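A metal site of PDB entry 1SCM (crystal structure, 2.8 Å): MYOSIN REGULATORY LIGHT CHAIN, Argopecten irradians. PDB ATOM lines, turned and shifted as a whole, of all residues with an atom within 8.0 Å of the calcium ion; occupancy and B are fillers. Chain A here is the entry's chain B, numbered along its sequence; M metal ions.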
ATOM      1  N   PHE A  13     -14.556 -17.090 -17.724  1.00  0.00           N
ATOM      2  CA  PHE A  13     -15.001 -15.852 -18.371  1.00  0.00           C
ATOM      3  C   PHE A  13     -16.523 -15.752 -18.393  1.00  0.00           C
ATOM      4  O   PHE A  13     -17.019 -14.629 -18.467  1.00  0.00           O
ATOM      5  CB  PHE A  13     -14.517 -15.791 -19.805  1.00  0.00           C
ATOM      6  CG  PHE A  13     -14.921 -14.503 -20.489  1.00  0.00           C
ATOM      7  CD1 PHE A  13     -14.112 -13.386 -20.350  1.00  0.00           C
ATOM      8  CD2 PHE A  13     -16.129 -14.417 -21.221  1.00  0.00           C
ATOM      9  CE1 PHE A  13     -14.493 -12.177 -20.927  1.00  0.00           C
ATOM     10  CE2 PHE A  13     -16.509 -13.208 -21.799  1.00  0.00           C
ATOM     11  CZ  PHE A  13     -15.697 -12.084 -21.653  1.00  0.00           C
ATOM     12  N   SER A  14     -17.241 -16.886 -18.356  1.00  0.00           N
ATOM     13  CA  SER A  14     -18.699 -16.898 -18.347  1.00  0.00           C
ATOM     14  C   SER A  14     -19.356 -16.494 -17.020  1.00  0.00           C
ATOM     15  O   SER A  14     -20.540 -16.106 -16.997  1.00  0.00           O
ATOM     16  CB  SER A  14     -19.182 -18.300 -18.713  1.00  0.00           C
ATOM     17  OG  SER A  14     -18.476 -18.798 -19.829  1.00  0.00           O
ATOM     18  N   MET A  15     -18.624 -16.565 -15.909  1.00  0.00           N
ATOM     19  CA  MET A  15     -19.164 -16.224 -14.608  1.00  0.00           C
ATOM     20  C   MET A  15     -18.813 -14.832 -14.169  1.00  0.00           C
ATOM     21  O   MET A  15     -19.665 -14.149 -13.608  1.00  0.00           O
ATOM     22  CB  MET A  15     -18.657 -17.205 -13.578  1.00  0.00           C
ATOM     23  CG  MET A  15     -19.301 -18.574 -13.720  1.00  0.00           C
ATOM     24  SD  MET A  15     -18.990 -19.692 -12.333  1.00  0.00           S
ATOM     25  CE  MET A  15     -19.188 -18.553 -10.976  1.00  0.00           C
ATOM     26  N   ILE A  16     -17.549 -14.446 -14.392  1.00  0.00           N
ATOM     27  CA  ILE A  16     -16.949 -13.129 -14.149  1.00  0.00           C
ATOM     28  C   ILE A  16     -17.860 -12.119 -14.863  1.00  0.00           C
ATOM     29  O   ILE A  16     -18.267 -11.072 -14.369  1.00  0.00           O
ATOM     30  CB  ILE A  16     -15.506 -13.152 -14.746  1.00  0.00           C
ATOM     31  CG1 ILE A  16     -14.662 -14.047 -13.875  1.00  0.00           C
ATOM     32  CG2 ILE A  16     -14.906 -11.771 -14.870  1.00  0.00           C
ATOM     33  CD1 ILE A  16     -13.253 -14.247 -14.433  1.00  0.00           C
ATOM     34  N   ASP A  17     -18.163 -12.487 -16.105  1.00  0.00           N
ATOM     35  CA  ASP A  17     -19.146 -11.801 -16.901  1.00  0.00           C
ATOM     36  C   ASP A  17     -20.380 -12.314 -16.236  1.00  0.00           C
ATOM     37  O   ASP A  17     -20.641 -13.513 -16.201  1.00  0.00           O
ATOM     38  CB  ASP A  17     -19.102 -12.271 -18.363  1.00  0.00           C
ATOM     39  CG  ASP A  17     -20.302 -11.976 -19.267  1.00  0.00           C
ATOM     40  OD1 ASP A  17     -21.396 -11.722 -18.768  1.00  0.00           O
ATOM     41  OD2 ASP A  17     -20.166 -11.955 -20.494  1.00  0.00           O
ATOM     42  N   VAL A  18     -21.107 -11.347 -15.714  1.00  0.00           N
ATOM     43  CA  VAL A  18     -22.443 -11.562 -15.178  1.00  0.00           C
ATOM     44  C   VAL A  18     -23.568 -11.189 -16.164  1.00  0.00           C
ATOM     45  O   VAL A  18     -24.479 -11.991 -16.362  1.00  0.00           O
ATOM     46  CB  VAL A  18     -22.484 -10.757 -13.859  1.00  0.00           C
ATOM     47  CG1 VAL A  18     -23.892 -10.540 -13.347  1.00  0.00           C
ATOM     48  CG2 VAL A  18     -21.731 -11.570 -12.831  1.00  0.00           C
ATOM     49  N   ASP A  19     -23.532 -10.016 -16.838  1.00  0.00           N
ATOM     50  CA  ASP A  19     -24.662  -9.532 -17.649  1.00  0.00           C
ATOM     51  C   ASP A  19     -24.870 -10.017 -19.061  1.00  0.00           C
ATOM     52  O   ASP A  19     -25.760  -9.555 -19.778  1.00  0.00           O
ATOM     53  CB  ASP A  19     -24.608  -8.029 -17.680  1.00  0.00           C
ATOM     54  CG  ASP A  19     -23.545  -7.358 -18.542  1.00  0.00           C
ATOM     55  OD1 ASP A  19     -22.462  -7.910 -18.798  1.00  0.00           O
ATOM     56  OD2 ASP A  19     -23.829  -6.250 -18.970  1.00  0.00           O
ATOM     57  N   ARG A  20     -24.029 -11.003 -19.402  1.00  0.00           N
ATOM     58  CA  ARG A  20     -23.919 -11.628 -20.705  1.00  0.00           C
ATOM     59  C   ARG A  20     -23.538 -10.800 -21.923  1.00  0.00           C
ATOM     60  O   ARG A  20     -23.278 -11.430 -22.944  1.00  0.00           O
ATOM     61  CB  ARG A  20     -25.201 -12.373 -21.096  1.00  0.00           C
ATOM     62  CG  ARG A  20     -25.192 -13.846 -20.686  1.00  0.00           C
ATOM     63  CD  ARG A  20     -26.166 -14.647 -21.555  1.00  0.00           C
ATOM     64  NE  ARG A  20     -27.573 -14.313 -21.344  1.00  0.00           N
ATOM     65  CZ  ARG A  20     -28.287 -13.535 -22.183  1.00  0.00           C
ATOM     66  NH1 ARG A  20     -27.774 -12.964 -23.281  1.00  0.00           N
ATOM     67  NH2 ARG A  20     -29.560 -13.356 -21.905  1.00  0.00           N
ATOM     68  N   ASP A  21     -23.385  -9.457 -21.865  1.00  0.00           N
ATOM     69  CA  ASP A  21     -23.002  -8.681 -23.050  1.00  0.00           C
ATOM     70  C   ASP A  21     -21.751  -9.165 -23.788  1.00  0.00           C
ATOM     71  O   ASP A  21     -21.542  -8.756 -24.935  1.00  0.00           O
ATOM     72  CB  ASP A  21     -22.812  -7.180 -22.707  1.00  0.00           C
ATOM     73  CG  ASP A  21     -21.778  -6.763 -21.650  1.00  0.00           C
ATOM     74  OD1 ASP A  21     -20.882  -7.500 -21.332  1.00  0.00           O
ATOM     75  OD2 ASP A  21     -21.867  -5.661 -21.115  1.00  0.00           O
ATOM     76  N   GLY A  22     -20.954 -10.037 -23.120  1.00  0.00           N
ATOM     77  CA  GLY A  22     -19.750 -10.644 -23.661  1.00  0.00           C
ATOM     78  C   GLY A  22     -18.464  -9.895 -23.333  1.00  0.00           C
ATOM     79  O   GLY A  22     -17.369 -10.328 -23.693  1.00  0.00           O
ATOM     80  N   PHE A  23     -18.566  -8.735 -22.687  1.00  0.00           N
ATOM     81  CA  PHE A  23     -17.379  -7.982 -22.314  1.00  0.00           C
ATOM     82  C   PHE A  23     -17.316  -7.884 -20.801  1.00  0.00           C
ATOM     83  O   PHE A  23     -18.359  -7.588 -20.220  1.00  0.00           O
ATOM     84  CB  PHE A  23     -17.428  -6.601 -22.924  1.00  0.00           C
ATOM     85  CG  PHE A  23     -17.556  -6.666 -24.436  1.00  0.00           C
ATOM     86  CD1 PHE A  23     -18.798  -6.934 -25.021  1.00  0.00           C
ATOM     87  CD2 PHE A  23     -16.432  -6.480 -25.221  1.00  0.00           C
ATOM     88  CE1 PHE A  23     -18.919  -7.014 -26.421  1.00  0.00           C
ATOM     89  CE2 PHE A  23     -16.557  -6.560 -26.603  1.00  0.00           C
ATOM     90  CZ  PHE A  23     -17.798  -6.819 -27.211  1.00  0.00           C
ATOM     91  N   VAL A  24     -16.228  -8.188 -20.096  1.00  0.00           N
ATOM     92  CA  VAL A  24     -16.198  -7.934 -18.671  1.00  0.00           C
ATOM     93  C   VAL A  24     -16.130  -6.406 -18.528  1.00  0.00           C
ATOM     94  O   VAL A  24     -15.271  -5.661 -18.996  1.00  0.00           O
ATOM     95  CB  VAL A  24     -14.982  -8.591 -18.017  1.00  0.00           C
ATOM     96  CG1 VAL A  24     -15.097  -8.453 -16.514  1.00  0.00           C
ATOM     97  CG2 VAL A  24     -14.927 -10.075 -18.305  1.00  0.00           C
ATOM     98  N   SER A  25     -17.271  -5.996 -17.978  1.00  0.00           N
ATOM     99  CA  SER A  25     -17.563  -4.605 -17.646  1.00  0.00           C
ATOM    100  C   SER A  25     -17.275  -4.470 -16.176  1.00  0.00           C
ATOM    101  O   SER A  25     -17.303  -5.475 -15.475  1.00  0.00           O
ATOM    102  CB  SER A  25     -19.051  -4.268 -17.880  1.00  0.00           C
ATOM    103  OG  SER A  25     -19.842  -5.270 -18.546  1.00  0.00           O
ATOM    104  N   LYS A  26     -16.992  -3.262 -15.676  1.00  0.00           N
ATOM    105  CA  LYS A  26     -16.730  -3.108 -14.239  1.00  0.00           C
ATOM    106  C   LYS A  26     -17.861  -3.559 -13.304  1.00  0.00           C
ATOM    107  O   LYS A  26     -17.675  -4.228 -12.280  1.00  0.00           O
ATOM    108  CB  LYS A  26     -16.385  -1.663 -13.963  1.00  0.00           C
ATOM    109  CG  LYS A  26     -15.899  -1.453 -12.545  1.00  0.00           C
ATOM    110  CD  LYS A  26     -16.101   0.003 -12.217  1.00  0.00           C
ATOM    111  CE  LYS A  26     -15.737   0.342 -10.787  1.00  0.00           C
ATOM    112  NZ  LYS A  26     -16.270   1.667 -10.523  1.00  0.00           N
ATOM    113  N   GLU A  27     -19.099  -3.307 -13.681  1.00  0.00           N
ATOM    114  CA  GLU A  27     -20.197  -3.636 -12.804  1.00  0.00           C
ATOM    115  C   GLU A  27     -20.357  -5.155 -12.617  1.00  0.00           C
ATOM    116  O   GLU A  27     -21.008  -5.560 -11.668  1.00  0.00           O
ATOM    117  CB  GLU A  27     -21.428  -2.952 -13.418  1.00  0.00           C
ATOM    118  CG  GLU A  27     -21.245  -1.449 -13.819  1.00  0.00           C
ATOM    119  CD  GLU A  27     -20.884  -1.109 -15.281  1.00  0.00           C
ATOM    120  OE1 GLU A  27     -21.599  -1.475 -16.221  1.00  0.00           O
ATOM    121  OE2 GLU A  27     -19.877  -0.416 -15.494  1.00  0.00           O
ATOM    122  N   ASP A  28     -19.741  -6.003 -13.490  1.00  0.00           N
ATOM    123  CA  ASP A  28     -19.797  -7.473 -13.417  1.00  0.00           C
ATOM    124  C   ASP A  28     -18.782  -8.014 -12.466  1.00  0.00           C
ATOM    125  O   ASP A  28     -19.019  -9.031 -11.812  1.00  0.00           O
ATOM    126  CB  ASP A  28     -19.434  -8.296 -14.656  1.00  0.00           C
ATOM    127  CG  ASP A  28     -20.090  -7.934 -15.963  1.00  0.00           C
ATOM    128  OD1 ASP A  28     -19.713  -6.906 -16.477  1.00  0.00           O
ATOM    129  OD2 ASP A  28     -20.958  -8.649 -16.484  1.00  0.00           O
ATOM    130  N   ILE A  29     -17.627  -7.357 -12.469  1.00  0.00           N
ATOM    131  CA  ILE A  29     -16.557  -7.756 -11.578  1.00  0.00           C
ATOM    132  C   ILE A  29     -17.104  -7.535 -10.161  1.00  0.00           C
ATOM    133  O   ILE A  29     -17.007  -8.415  -9.318  1.00  0.00           O
ATOM    134  CB  ILE A  29     -15.259  -6.900 -11.768  1.00  0.00           C
ATOM    135  CG1 ILE A  29     -14.867  -6.578 -13.184  1.00  0.00           C
ATOM    136  CG2 ILE A  29     -14.152  -7.778 -11.216  1.00  0.00           C
ATOM    137  CD1 ILE A  29     -13.642  -5.649 -13.201  1.00  0.00           C
ATOM    138  N   LEU A  56     -13.029  -5.486 -22.596  1.00  0.00           N
ATOM    139  CA  LEU A  56     -12.648  -6.815 -22.154  1.00  0.00           C
ATOM    140  C   LEU A  56     -13.467  -7.921 -22.825  1.00  0.00           C
ATOM    141  O   LEU A  56     -14.413  -8.502 -22.295  1.00  0.00           O
ATOM    142  CB  LEU A  56     -12.778  -6.896 -20.640  1.00  0.00           C
ATOM    143  CG  LEU A  56     -11.530  -6.678 -19.821  1.00  0.00           C
ATOM    144  CD1 LEU A  56     -11.880  -6.177 -18.429  1.00  0.00           C
ATOM    145  CD2 LEU A  56     -10.764  -7.980 -19.767  1.00  0.00           C
HETATM  146 CA    CA M   1     -20.165  -9.148 -19.467  1.00  0.00          CA
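OD1 of Asp 17 lies within hydrogen-bond range of N of Arg 20. N of Val 18 sits at hydrogen-bond distance from OD2 of Asp 28, 2.8 Å away. OD1 of Asp 28 sits at hydrogen-bond distance from OG of Ser 25 (2.6 Å). The backbone NH of Asp 19 is in hydrogen-bond range of the side-chain carboxylate of Asp 28. The backbone carbonyl oxygen of Phe 23 lies close to the side-chain hydroxyl of Ser 25, at 3.2 Å. OD1 of Asp 17 is in hydrogen-bond range of N of Asp 19. OD2 of Asp 17 is in hydrogen-bond range of N of Gly 22. OD2 of Asp 21 lies within hydrogen-bond range of OG of Ser 25 (3.3 Å).
Merely in contact with the calcium ion: Gly 22 (3.8 Å) and Ser 25 (3.999 Å). Of the 18 residues printed, 7 come within 4 Å of the calcium ion.
The calcium ion is bound by the backbone carbonyl oxygen of Phe 23 (2.5 Å), the side-chain carboxylate of Asp 21 (2.6 Å) and the side-chain carboxylate of Asp 19 (2.7 Å). The calcium ion has three donor atoms within binding distance. Slightly farther from the calcium ion lies OD1 of Asp 17 (2.9 Å). Slightly farther from the calcium ion lies the side-chain carboxylate (OD2) of Asp 17 (3.0 Å). Slightly farther from the calcium ion lies OD2 of Asp 28 (3.1 Å).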
